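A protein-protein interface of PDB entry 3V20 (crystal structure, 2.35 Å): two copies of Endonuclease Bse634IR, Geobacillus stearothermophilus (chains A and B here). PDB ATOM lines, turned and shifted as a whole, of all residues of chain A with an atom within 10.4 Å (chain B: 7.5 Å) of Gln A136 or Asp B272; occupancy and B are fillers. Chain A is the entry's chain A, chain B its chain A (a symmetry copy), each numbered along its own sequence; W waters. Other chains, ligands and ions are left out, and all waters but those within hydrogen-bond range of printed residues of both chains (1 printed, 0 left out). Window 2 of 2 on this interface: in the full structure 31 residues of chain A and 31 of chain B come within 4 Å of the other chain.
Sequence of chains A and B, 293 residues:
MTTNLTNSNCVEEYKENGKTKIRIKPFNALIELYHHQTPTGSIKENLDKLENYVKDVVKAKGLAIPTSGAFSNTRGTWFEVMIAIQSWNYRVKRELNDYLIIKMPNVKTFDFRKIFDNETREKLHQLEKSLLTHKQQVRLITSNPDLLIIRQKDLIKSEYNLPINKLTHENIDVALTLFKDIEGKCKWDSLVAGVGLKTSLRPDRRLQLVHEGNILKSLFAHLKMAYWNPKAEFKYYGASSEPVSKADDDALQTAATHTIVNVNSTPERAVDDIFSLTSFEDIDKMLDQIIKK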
ATOM      1  N   GLU A 128       7.618  24.345   5.180  1.00  0.00           N
ATOM      2  CA  GLU A 128       7.725  24.203   3.720  1.00  0.00           C
ATOM      3  C   GLU A 128       7.927  22.744   3.312  1.00  0.00           C
ATOM      4  O   GLU A 128       7.262  22.243   2.396  1.00  0.00           O
ATOM      5  CB  GLU A 128       8.859  25.092   3.154  1.00  0.00           C
ATOM      6  CG  GLU A 128       9.476  24.600   1.812  1.00  0.00           C
ATOM      7  CD  GLU A 128      10.701  25.399   1.349  1.00  0.00           C
ATOM      8  OE1 GLU A 128      11.431  25.962   2.198  1.00  0.00           O
ATOM      9  OE2 GLU A 128      10.937  25.456   0.120  1.00  0.00           O
ATOM     10  N   LYS A 129       8.845  22.073   4.001  1.00  0.00           N
ATOM     11  CA  LYS A 129       9.157  20.673   3.726  1.00  0.00           C
ATOM     12  C   LYS A 129       7.966  19.762   4.045  1.00  0.00           C
ATOM     13  O   LYS A 129       7.698  18.819   3.303  1.00  0.00           O
ATOM     14  CB  LYS A 129      10.410  20.241   4.494  1.00  0.00           C
ATOM     15  CG  LYS A 129      11.169  19.055   3.894  1.00  0.00           C
ATOM     16  CD  LYS A 129      12.466  18.795   4.670  1.00  0.00           C
ATOM     17  CE  LYS A 129      13.112  17.459   4.290  1.00  0.00           C
ATOM     18  NZ  LYS A 129      14.402  17.238   5.000  1.00  0.00           N
ATOM     19  N   SER A 130       7.238  20.053   5.125  1.00  0.00           N
ATOM     20  CA  SER A 130       6.096  19.213   5.505  1.00  0.00           C
ATOM     21  C   SER A 130       4.916  19.370   4.543  1.00  0.00           C
ATOM     22  O   SER A 130       4.136  18.433   4.348  1.00  0.00           O
ATOM     23  CB  SER A 130       5.656  19.470   6.950  1.00  0.00           C
ATOM     24  OG  SER A 130       4.705  20.518   7.021  1.00  0.00           O
ATOM     25  N   LEU A 131       4.799  20.550   3.939  1.00  0.00           N
ATOM     26  CA  LEU A 131       3.699  20.836   3.024  1.00  0.00           C
ATOM     27  C   LEU A 131       3.859  20.144   1.666  1.00  0.00           C
ATOM     28  O   LEU A 131       2.888  20.002   0.921  1.00  0.00           O
ATOM     29  CB  LEU A 131       3.513  22.345   2.848  1.00  0.00           C
ATOM     30  CG  LEU A 131       3.026  23.182   4.034  1.00  0.00           C
ATOM     31  CD1 LEU A 131       2.876  24.638   3.611  1.00  0.00           C
ATOM     32  CD2 LEU A 131       1.719  22.653   4.633  1.00  0.00           C
ATOM     33  N   LEU A 132       5.084  19.714   1.360  1.00  0.00           N
ATOM     34  CA  LEU A 132       5.391  18.990   0.122  1.00  0.00           C
ATOM     35  C   LEU A 132       5.367  17.462   0.316  1.00  0.00           C
ATOM     36  O   LEU A 132       5.236  16.709  -0.649  1.00  0.00           O
ATOM     37  CB  LEU A 132       6.752  19.426  -0.433  1.00  0.00           C
ATOM     38  CG  LEU A 132       6.955  20.833  -1.008  1.00  0.00           C
ATOM     39  CD1 LEU A 132       8.437  21.175  -1.089  1.00  0.00           C
ATOM     40  CD2 LEU A 132       6.319  20.968  -2.371  1.00  0.00           C
ATOM     41  N   THR A 133       5.497  17.023   1.566  1.00  0.00           N
ATOM     42  CA  THR A 133       5.465  15.604   1.934  1.00  0.00           C
ATOM     43  C   THR A 133       4.014  15.089   2.008  1.00  0.00           C
ATOM     44  O   THR A 133       3.533  14.686   3.073  1.00  0.00           O
ATOM     45  CB  THR A 133       6.192  15.364   3.291  1.00  0.00           C
ATOM     46  OG1 THR A 133       7.371  16.176   3.357  1.00  0.00           O
ATOM     47  CG2 THR A 133       6.588  13.895   3.462  1.00  0.00           C
ATOM     48  N   HIS A 134       3.324  15.141   0.868  1.00  0.00           N
ATOM     49  CA  HIS A 134       1.952  14.643   0.713  1.00  0.00           C
ATOM     50  C   HIS A 134       1.734  14.279  -0.752  1.00  0.00           C
ATOM     51  O   HIS A 134       2.466  14.755  -1.627  1.00  0.00           O
ATOM     52  CB  HIS A 134       0.918  15.693   1.155  1.00  0.00           C
ATOM     53  CG  HIS A 134       0.858  15.895   2.638  1.00  0.00           C
ATOM     54  ND1 HIS A 134       1.414  16.992   3.264  1.00  0.00           N
ATOM     55  CD2 HIS A 134       0.330  15.127   3.621  1.00  0.00           C
ATOM     56  CE1 HIS A 134       1.229  16.890   4.568  1.00  0.00           C
ATOM     57  NE2 HIS A 134       0.568  15.771   4.811  1.00  0.00           N
ATOM     58  N   LYS A 135       0.742  13.432  -1.020  1.00  0.00           N
ATOM     59  CA  LYS A 135       0.391  13.074  -2.397  1.00  0.00           C
ATOM     60  C   LYS A 135       0.143  14.312  -3.268  1.00  0.00           C
ATOM     61  O   LYS A 135       0.639  14.386  -4.397  1.00  0.00           O
ATOM     62  CB  LYS A 135      -0.788  12.085  -2.449  1.00  0.00           C
ATOM     63  CG  LYS A 135      -1.785  12.199  -1.300  1.00  0.00           C
ATOM     64  CD  LYS A 135      -2.280  10.816  -0.843  1.00  0.00           C
ATOM     65  CE  LYS A 135      -2.955  10.888   0.540  1.00  0.00           C
ATOM     66  NZ  LYS A 135      -3.183   9.530   1.148  1.00  0.00           N
ATOM     67  N   GLN A 136      -0.604  15.282  -2.733  1.00  0.00           N
ATOM     68  CA  GLN A 136      -0.828  16.567  -3.404  1.00  0.00           C
ATOM     69  C   GLN A 136       0.124  17.621  -2.829  1.00  0.00           C
ATOM     70  O   GLN A 136      -0.094  18.099  -1.714  1.00  0.00           O
ATOM     71  CB  GLN A 136      -2.286  17.019  -3.227  1.00  0.00           C
ATOM     72  CG  GLN A 136      -2.684  18.198  -4.129  1.00  0.00           C
ATOM     73  CD  GLN A 136      -4.081  18.754  -3.842  1.00  0.00           C
ATOM     74  OE1 GLN A 136      -4.962  18.718  -4.708  1.00  0.00           O
ATOM     75  NE2 GLN A 136      -4.280  19.288  -2.638  1.00  0.00           N
ATOM     76  N   GLN A 137       1.174  17.968  -3.579  1.00  0.00           N
ATOM     77  CA  GLN A 137       2.167  18.971  -3.136  1.00  0.00           C
ATOM     78  C   GLN A 137       1.559  20.362  -2.953  1.00  0.00           C
ATOM     79  O   GLN A 137       0.908  20.876  -3.861  1.00  0.00           O
ATOM     80  CB  GLN A 137       3.332  19.074  -4.133  1.00  0.00           C
ATOM     81  CG  GLN A 137       4.377  17.972  -4.024  1.00  0.00           C
ATOM     82  CD  GLN A 137       5.718  18.381  -4.615  1.00  0.00           C
ATOM     83  OE1 GLN A 137       5.786  19.083  -5.623  1.00  0.00           O
ATOM     84  NE2 GLN A 137       6.797  17.944  -3.977  1.00  0.00           N
ATOM     85  N   VAL A 138       1.765  20.970  -1.786  1.00  0.00           N
ATOM     86  CA  VAL A 138       1.318  22.357  -1.580  1.00  0.00           C
ATOM     87  C   VAL A 138       2.452  23.280  -1.106  1.00  0.00           C
ATOM     88  O   VAL A 138       3.423  22.826  -0.492  1.00  0.00           O
ATOM     89  CB  VAL A 138       0.024  22.480  -0.683  1.00  0.00           C
ATOM     90  CG1 VAL A 138      -0.752  21.169  -0.644  1.00  0.00           C
ATOM     91  CG2 VAL A 138       0.336  22.927   0.719  1.00  0.00           C
ATOM     92  N   ARG A 139       2.316  24.569  -1.416  1.00  0.00           N
ATOM     93  CA  ARG A 139       3.288  25.596  -1.047  1.00  0.00           C
ATOM     94  C   ARG A 139       2.590  26.786  -0.376  1.00  0.00           C
ATOM     95  O   ARG A 139       1.372  26.771  -0.189  1.00  0.00           O
ATOM     96  CB  ARG A 139       4.017  26.084  -2.301  1.00  0.00           C
ATOM     97  CG  ARG A 139       4.801  25.021  -3.034  1.00  0.00           C
ATOM     98  CD  ARG A 139       5.291  25.530  -4.376  1.00  0.00           C
ATOM     99  NE  ARG A 139       5.771  24.447  -5.233  1.00  0.00           N
ATOM    100  CZ  ARG A 139       6.989  23.917  -5.171  1.00  0.00           C
ATOM    101  NH1 ARG A 139       7.875  24.360  -4.281  1.00  0.00           N
ATOM    102  NH2 ARG A 139       7.322  22.937  -5.997  1.00  0.00           N
ATOM    103  N   VAL B 192     -20.059  21.536  -7.291  1.00  0.00           N
ATOM    104  CA  VAL B 192     -18.927  20.603  -7.206  1.00  0.00           C
ATOM    105  C   VAL B 192     -17.573  21.184  -7.601  1.00  0.00           C
ATOM    106  O   VAL B 192     -16.543  20.753  -7.084  1.00  0.00           O
ATOM    107  CB  VAL B 192     -19.207  19.234  -7.914  1.00  0.00           C
ATOM    108  CG1 VAL B 192     -20.411  18.525  -7.249  1.00  0.00           C
ATOM    109  CG2 VAL B 192     -19.421  19.390  -9.414  1.00  0.00           C
ATOM    110  N   ALA B 193     -17.561  22.165  -8.497  1.00  0.00           N
ATOM    111  CA  ALA B 193     -16.311  22.831  -8.872  1.00  0.00           C
ATOM    112  C   ALA B 193     -16.539  24.214  -9.427  1.00  0.00           C
ATOM    113  O   ALA B 193     -17.631  24.513  -9.891  1.00  0.00           O
ATOM    114  CB  ALA B 193     -15.510  21.983  -9.861  1.00  0.00           C
ATOM    115  N   GLY B 194     -15.509  25.058  -9.356  1.00  0.00           N
ATOM    116  CA  GLY B 194     -15.490  26.345 -10.069  1.00  0.00           C
ATOM    117  C   GLY B 194     -14.225  26.499 -10.905  1.00  0.00           C
ATOM    118  O   GLY B 194     -13.215  25.816 -10.656  1.00  0.00           O
ATOM    119  N   GLY B 213     -10.123  30.727  -4.905  1.00  0.00           N
ATOM    120  CA  GLY B 213     -10.260  29.360  -4.443  1.00  0.00           C
ATOM    121  C   GLY B 213     -10.192  29.256  -2.931  1.00  0.00           C
ATOM    122  O   GLY B 213     -10.908  28.452  -2.323  1.00  0.00           O
ATOM    123  N   LYS B 217     -13.521  27.899  -0.858  1.00  0.00           N
ATOM    124  CA  LYS B 217     -13.328  26.672  -0.112  1.00  0.00           C
ATOM    125  C   LYS B 217     -13.597  26.915   1.362  1.00  0.00           C
ATOM    126  O   LYS B 217     -13.948  25.995   2.105  1.00  0.00           O
ATOM    127  CB  LYS B 217     -11.909  26.121  -0.317  1.00  0.00           C
ATOM    128  CG  LYS B 217     -11.729  25.460  -1.661  1.00  0.00           C
ATOM    129  CD  LYS B 217     -10.359  24.841  -1.876  1.00  0.00           C
ATOM    130  CE  LYS B 217     -10.387  24.079  -3.198  1.00  0.00           C
ATOM    131  NZ  LYS B 217      -9.253  23.142  -3.319  1.00  0.00           N
ATOM    132  N   PHE B 234     -15.486  20.479  -2.756  1.00  0.00           N
ATOM    133  CA  PHE B 234     -15.530  21.529  -3.758  1.00  0.00           C
ATOM    134  C   PHE B 234     -14.111  21.745  -4.264  1.00  0.00           C
ATOM    135  O   PHE B 234     -13.182  21.902  -3.486  1.00  0.00           O
ATOM    136  CB  PHE B 234     -16.130  22.840  -3.206  1.00  0.00           C
ATOM    137  CG  PHE B 234     -16.110  23.993  -4.206  1.00  0.00           C
ATOM    138  CD1 PHE B 234     -17.057  24.076  -5.221  1.00  0.00           C
ATOM    139  CD2 PHE B 234     -15.133  24.982  -4.135  1.00  0.00           C
ATOM    140  CE1 PHE B 234     -17.040  25.129  -6.146  1.00  0.00           C
ATOM    141  CE2 PHE B 234     -15.107  26.035  -5.062  1.00  0.00           C
ATOM    142  CZ  PHE B 234     -16.061  26.107  -6.065  1.00  0.00           C
ATOM    143  N   LYS B 235     -13.949  21.728  -5.578  1.00  0.00           N
ATOM    144  CA  LYS B 235     -12.636  21.897  -6.183  1.00  0.00           C
ATOM    145  C   LYS B 235     -12.608  23.171  -6.999  1.00  0.00           C
ATOM    146  O   LYS B 235     -13.619  23.591  -7.547  1.00  0.00           O
ATOM    147  CB  LYS B 235     -12.293  20.678  -7.046  1.00  0.00           C
ATOM    148  CG  LYS B 235     -11.693  19.507  -6.273  1.00  0.00           C
ATOM    149  CD  LYS B 235     -11.400  18.356  -7.224  1.00  0.00           C
ATOM    150  CE  LYS B 235     -10.269  17.439  -6.750  1.00  0.00           C
ATOM    151  NZ  LYS B 235     -10.545  16.820  -5.411  1.00  0.00           N
ATOM    152  N   TYR B 236     -11.447  23.798  -7.085  1.00  0.00           N
ATOM    153  CA  TYR B 236     -11.320  25.026  -7.856  1.00  0.00           C
ATOM    154  C   TYR B 236     -10.128  24.955  -8.785  1.00  0.00           C
ATOM    155  O   TYR B 236      -9.078  24.448  -8.392  1.00  0.00           O
ATOM    156  CB  TYR B 236     -11.203  26.226  -6.928  1.00  0.00           C
ATOM    157  CG  TYR B 236     -11.239  27.546  -7.651  1.00  0.00           C
ATOM    158  CD1 TYR B 236     -12.442  28.047  -8.156  1.00  0.00           C
ATOM    159  CD2 TYR B 236     -10.072  28.291  -7.849  1.00  0.00           C
ATOM    160  CE1 TYR B 236     -12.487  29.260  -8.824  1.00  0.00           C
ATOM    161  CE2 TYR B 236     -10.111  29.517  -8.524  1.00  0.00           C
ATOM    162  CZ  TYR B 236     -11.323  29.988  -9.001  1.00  0.00           C
ATOM    163  OH  TYR B 236     -11.396  31.192  -9.660  1.00  0.00           O
ATOM    164  N   TYR B 237     -10.300  25.496  -9.996  1.00  0.00           N
ATOM    165  CA  TYR B 237      -9.360  25.346 -11.101  1.00  0.00           C
ATOM    166  C   TYR B 237      -9.078  26.652 -11.831  1.00  0.00           C
ATOM    167  O   TYR B 237      -9.923  27.545 -11.888  1.00  0.00           O
ATOM    168  CB  TYR B 237      -9.939  24.363 -12.132  1.00  0.00           C
ATOM    169  CG  TYR B 237     -10.211  22.968 -11.592  1.00  0.00           C
ATOM    170  CD1 TYR B 237      -9.179  22.024 -11.501  1.00  0.00           C
ATOM    171  CD2 TYR B 237     -11.491  22.599 -11.162  1.00  0.00           C
ATOM    172  CE1 TYR B 237      -9.408  20.746 -10.990  1.00  0.00           C
ATOM    173  CE2 TYR B 237     -11.737  21.323 -10.659  1.00  0.00           C
ATOM    174  CZ  TYR B 237     -10.680  20.398 -10.585  1.00  0.00           C
ATOM    175  OH  TYR B 237     -10.890  19.128 -10.104  1.00  0.00           O
ATOM    176  N   GLY B 238      -7.891  26.747 -12.419  1.00  0.00           N
ATOM    177  CA  GLY B 238      -7.561  27.855 -13.300  1.00  0.00           C
ATOM    178  C   GLY B 238      -7.397  27.379 -14.729  1.00  0.00           C
ATOM    179  O   GLY B 238      -7.076  26.195 -14.970  1.00  0.00           O
ATOM    180  N   LEU B 252       0.382  28.560  -8.165  1.00  0.00           N
ATOM    181  CA  LEU B 252      -0.944  27.986  -8.057  1.00  0.00           C
ATOM    182  C   LEU B 252      -0.964  26.667  -7.254  1.00  0.00           C
ATOM    183  O   LEU B 252      -1.998  26.012  -7.158  1.00  0.00           O
ATOM    184  CB  LEU B 252      -1.579  27.846  -9.439  1.00  0.00           C
ATOM    185  CG  LEU B 252      -1.754  29.159 -10.244  1.00  0.00           C
ATOM    186  CD1 LEU B 252      -1.907  28.883 -11.720  1.00  0.00           C
ATOM    187  CD2 LEU B 252      -2.954  29.952  -9.761  1.00  0.00           C
ATOM    188  N   GLN B 253       0.174  26.298  -6.661  1.00  0.00           N
ATOM    189  CA  GLN B 253       0.218  25.209  -5.663  1.00  0.00           C
ATOM    190  C   GLN B 253      -0.007  25.703  -4.229  1.00  0.00           C
ATOM    191  O   GLN B 253       0.086  24.925  -3.270  1.00  0.00           O
ATOM    192  CB  GLN B 253       1.536  24.438  -5.740  1.00  0.00           C
ATOM    193  CG  GLN B 253       1.539  23.314  -6.750  1.00  0.00           C
ATOM    194  CD  GLN B 253       2.932  22.817  -7.060  1.00  0.00           C
ATOM    195  OE1 GLN B 253       3.869  23.045  -6.303  1.00  0.00           O
ATOM    196  NE2 GLN B 253       3.074  22.130  -8.179  1.00  0.00           N
ATOM    197  N   THR B 254      -0.327  26.989  -4.089  1.00  0.00           N
ATOM    198  CA  THR B 254      -0.469  27.616  -2.777  1.00  0.00           C
ATOM    199  C   THR B 254      -1.657  27.081  -1.974  1.00  0.00           C
ATOM    200  O   THR B 254      -2.772  26.936  -2.494  1.00  0.00           O
ATOM    201  CB  THR B 254      -0.495  29.136  -2.916  1.00  0.00           C
ATOM    202  OG1 THR B 254       0.774  29.550  -3.433  1.00  0.00           O
ATOM    203  CG2 THR B 254      -0.717  29.835  -1.578  1.00  0.00           C
ATOM    204  N   THR B 266      -4.471  17.356   6.578  1.00  0.00           N
ATOM    205  CA  THR B 266      -4.066  17.206   5.186  1.00  0.00           C
ATOM    206  C   THR B 266      -4.171  18.565   4.461  1.00  0.00           C
ATOM    207  O   THR B 266      -5.280  19.065   4.234  1.00  0.00           O
ATOM    208  CB  THR B 266      -4.904  16.112   4.466  1.00  0.00           C
ATOM    209  OG1 THR B 266      -4.656  14.842   5.083  1.00  0.00           O
ATOM    210  CG2 THR B 266      -4.534  16.010   2.991  1.00  0.00           C
ATOM    211  N   PRO B 267      -3.013  19.173   4.124  1.00  0.00           N
ATOM    212  CA  PRO B 267      -2.961  20.407   3.342  1.00  0.00           C
ATOM    213  C   PRO B 267      -3.784  20.315   2.054  1.00  0.00           C
ATOM    214  O   PRO B 267      -3.731  19.310   1.345  1.00  0.00           O
ATOM    215  CB  PRO B 267      -1.477  20.529   2.989  1.00  0.00           C
ATOM    216  CG  PRO B 267      -0.775  19.785   4.049  1.00  0.00           C
ATOM    217  CD  PRO B 267      -1.662  18.644   4.382  1.00  0.00           C
ATOM    218  N   GLU B 268      -4.547  21.361   1.766  1.00  0.00           N
ATOM    219  CA  GLU B 268      -5.293  21.446   0.518  1.00  0.00           C
ATOM    220  C   GLU B 268      -4.848  22.671  -0.293  1.00  0.00           C
ATOM    221  O   GLU B 268      -4.663  23.752   0.266  1.00  0.00           O
ATOM    222  CB  GLU B 268      -6.782  21.508   0.831  1.00  0.00           C
ATOM    223  CG  GLU B 268      -7.694  21.442  -0.370  1.00  0.00           C
ATOM    224  CD  GLU B 268      -9.159  21.575   0.012  1.00  0.00           C
ATOM    225  OE1 GLU B 268      -9.454  21.547   1.239  1.00  0.00           O
ATOM    226  OE2 GLU B 268     -10.003  21.702  -0.922  1.00  0.00           O
ATOM    227  N   ARG B 269      -4.648  22.480  -1.598  1.00  0.00           N
ATOM    228  CA  ARG B 269      -4.335  23.570  -2.533  1.00  0.00           C
ATOM    229  C   ARG B 269      -5.582  24.437  -2.698  1.00  0.00           C
ATOM    230  O   ARG B 269      -6.702  23.916  -2.701  1.00  0.00           O
ATOM    231  CB  ARG B 269      -3.917  23.018  -3.904  1.00  0.00           C
ATOM    232  CG  ARG B 269      -2.495  22.437  -3.971  1.00  0.00           C
ATOM    233  CD  ARG B 269      -2.101  21.947  -5.373  1.00  0.00           C
ATOM    234  NE  ARG B 269      -2.421  22.926  -6.423  1.00  0.00           N
ATOM    235  CZ  ARG B 269      -2.186  22.758  -7.729  1.00  0.00           C
ATOM    236  NH1 ARG B 269      -1.601  21.646  -8.188  1.00  0.00           N
ATOM    237  NH2 ARG B 269      -2.525  23.716  -8.583  1.00  0.00           N
ATOM    238  N   ALA B 270      -5.395  25.748  -2.821  1.00  0.00           N
ATOM    239  CA  ALA B 270      -6.523  26.642  -3.116  1.00  0.00           C
ATOM    240  C   ALA B 270      -7.036  26.417  -4.555  1.00  0.00           C
ATOM    241  O   ALA B 270      -8.246  26.416  -4.802  1.00  0.00           O
ATOM    242  CB  ALA B 270      -6.144  28.102  -2.901  1.00  0.00           C
ATOM    243  N   VAL B 271      -6.101  26.214  -5.482  1.00  0.00           N
ATOM    244  CA  VAL B 271      -6.429  25.916  -6.871  1.00  0.00           C
ATOM    245  C   VAL B 271      -5.942  24.503  -7.115  1.00  0.00           C
ATOM    246  O   VAL B 271      -4.739  24.235  -7.074  1.00  0.00           O
ATOM    247  CB  VAL B 271      -5.777  26.940  -7.863  1.00  0.00           C
ATOM    248  CG1 VAL B 271      -6.218  26.698  -9.287  1.00  0.00           C
ATOM    249  CG2 VAL B 271      -6.116  28.376  -7.458  1.00  0.00           C
ATOM    250  N   ASP B 272      -6.882  23.593  -7.345  1.00  0.00           N
ATOM    251  CA  ASP B 272      -6.562  22.183  -7.433  1.00  0.00           C
ATOM    252  C   ASP B 272      -5.723  21.866  -8.666  1.00  0.00           C
ATOM    253  O   ASP B 272      -4.891  20.972  -8.616  1.00  0.00           O
ATOM    254  CB  ASP B 272      -7.833  21.334  -7.373  1.00  0.00           C
ATOM    255  CG  ASP B 272      -8.456  21.322  -5.986  1.00  0.00           C
ATOM    256  OD1 ASP B 272      -7.967  20.557  -5.121  1.00  0.00           O
ATOM    257  OD2 ASP B 272      -9.425  22.080  -5.753  1.00  0.00           O
ATOM    258  N   ASP B 273      -5.914  22.622  -9.747  1.00  0.00           N
ATOM    259  CA  ASP B 273      -5.168  22.392 -10.984  1.00  0.00           C
ATOM    260  C   ASP B 273      -5.305  23.597 -11.935  1.00  0.00           C
ATOM    261  O   ASP B 273      -6.236  24.397 -11.807  1.00  0.00           O
ATOM    262  CB  ASP B 273      -5.647  21.085 -11.640  1.00  0.00           C
ATOM    263  CG  ASP B 273      -4.570  20.393 -12.480  1.00  0.00           C
ATOM    264  OD1 ASP B 273      -3.492  20.966 -12.707  1.00  0.00           O
ATOM    265  OD2 ASP B 273      -4.814  19.258 -12.948  1.00  0.00           O
ATOM    266  N   ILE B 274      -4.351  23.731 -12.861  1.00  0.00           N
ATOM    267  CA  ILE B 274      -4.317  24.823 -13.840  1.00  0.00           C
ATOM    268  C   ILE B 274      -4.178  24.201 -15.216  1.00  0.00           C
ATOM    269  O   ILE B 274      -3.287  23.379 -15.450  1.00  0.00           O
ATOM    270  CB  ILE B 274      -3.162  25.835 -13.570  1.00  0.00           C
ATOM    271  CG1 ILE B 274      -2.947  26.793 -14.757  1.00  0.00           C
ATOM    272  CG2 ILE B 274      -1.850  25.119 -13.242  1.00  0.00           C
ATOM    273  CD1 ILE B 274      -3.869  28.030 -14.764  1.00  0.00           C
ATOM    274  N   PHE B 275      -5.070  24.590 -16.115  1.00  0.00           N
ATOM    275  CA  PHE B 275      -5.128  24.034 -17.468  1.00  0.00           C
ATOM    276  C   PHE B 275      -4.665  25.040 -18.503  1.00  0.00           C
ATOM    277  O   PHE B 275      -5.039  26.210 -18.459  1.00  0.00           O
ATOM    278  CB  PHE B 275      -6.559  23.618 -17.830  1.00  0.00           C
ATOM    279  CG  PHE B 275      -7.113  22.557 -16.949  1.00  0.00           C
ATOM    280  CD1 PHE B 275      -7.028  21.221 -17.318  1.00  0.00           C
ATOM    281  CD2 PHE B 275      -7.723  22.889 -15.748  1.00  0.00           C
ATOM    282  CE1 PHE B 275      -7.547  20.233 -16.496  1.00  0.00           C
ATOM    283  CE2 PHE B 275      -8.237  21.908 -14.917  1.00  0.00           C
ATOM    284  CZ  PHE B 275      -8.148  20.587 -15.283  1.00  0.00           C
ATOM    285  N   GLN B 289     -11.655  16.069 -16.814  1.00  0.00           N
ATOM    286  CA  GLN B 289     -10.932  15.857 -15.562  1.00  0.00           C
ATOM    287  C   GLN B 289     -11.722  16.392 -14.372  1.00  0.00           C
ATOM    288  O   GLN B 289     -11.724  15.797 -13.297  1.00  0.00           O
ATOM    289  CB  GLN B 289      -9.536  16.488 -15.609  1.00  0.00           C
ATOM    290  CG  GLN B 289      -8.669  16.109 -14.403  1.00  0.00           C
ATOM    291  CD  GLN B 289      -7.418  16.944 -14.273  1.00  0.00           C
ATOM    292  OE1 GLN B 289      -7.306  17.779 -13.364  1.00  0.00           O
ATOM    293  NE2 GLN B 289      -6.462  16.723 -15.174  1.00  0.00           N
HETATM  294  O   HOH W   1      -2.094  17.544   0.842  1.00  0.00           O
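The backbone carbonyl oxygen (O) of Ser A130 lies within hydrogen-bond range of a ring nitrogen (ND1) of His A134 (3.3 Å).
NZ of Lys B217 is in hydrogen-bond range of O of Arg B269 (2.7 Å).
The guanidinium group (NH1) of Arg B269 lies close to the backbone carbonyl oxygen (O) of Asp B272 (3.4 Å).
The backbone carbonyl oxygen of Thr B254 lies within hydrogen-bond range of the backbone NH of Ala B270, 2.9 Å away.
The side-chain amino group of Lys B217 lies within salt-bridge range of the side-chain carboxylate of Glu B268 (2.9 Å).
The guanidinium group (NH2) of Arg B269 is in hydrogen-bond range of the backbone carbonyl oxygen (O) of Leu B252.
Water W1 bridges the backbone carbonyl oxygen of Pro B267 and the backbone carbonyl oxygen of Gln A136.
No position is printed for both chains.
Of the 12 pairs that touch across the chains among the printed residues, none has its exchanged pair printed and touching as well.
Leu A131 touches Pro B267 (CD2 to CG, 3.8 Å).
His A134 touches Pro B267 (CE1 to CD, 3.4 Å).
Gln A136 touches Glu B268.
Asp B272 touches Gln A136.
Gln B253 touches Gln A137 (CG to O, 3.8 Å).
Gln A137 touches Arg B269.
CA of Val A138 touches O of Gln B253, 3.3 Å away.
Pro B267 touches Val A138.
Val A138 touches Arg B269 (CG1 to CG, 3.96 Å).
O of Arg A139 touches CA of Thr B254, 3.3 Å away.
Of the 12 printed residues of chain A, 6 touch a printed residue of chain B.
Printed residues of chain A that touch a printed residue of chain B: Leu A131, His A134, Gln A136, Gln A137, Val A138 and Arg A139.
Hydrophobic or aromatic side chains of chain A within 4 Å of the printed part of chain B: Leu A131, His A134 and Val A138.
Of the 24 printed residues of chain B, 6 touch a printed residue of chain A.
Hydrophobic or aromatic side chains of chain B within 4 Å of the printed part of chain A: Pro B267.
Among the printed residues, no Asp or Glu carboxylate lies within 4 Å of a Lys or Arg side-chain nitrogen of the other chain.
NE2 of Gln A136 sits close to N of Arg B269.
The side-chain amide oxygen of Gln B253 lies within hydrogen-bond range of the guanidinium group of Arg A139 (2.6 Å).
Of chain B, only Glu B268 (3.96 Å), Arg B269 (3.4 Å) and Asp B272 (3.5 Å) come within 4 Å of Gln A136.
No residue of chain A comes within 4 Å of Lys B235.
Printed residues of chain A within 4 Å of Gln B253: Gln A137, Val A138 and Arg A139.
Printed residues of chain A within 4 Å of Pro B267: Leu A131, His A134 and Val A138.
No residue of chain A comes within 4 Å of Val B271.
Of chain A, only Gln A136 comes within 4 Å of Asp B272.
Asp B273 touches none of the printed residues of chain A.
Ile B274 touches none of the printed residues of chain A.
Phe B275 touches none of the printed residues of chain A.
The nearest residue of chain A that does not touch Asp B272 is Gln A137 (7.5 Å).
The nearest printed residue of chain A that does not touch Pro B267 is Gln A136 (4.02 Å).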
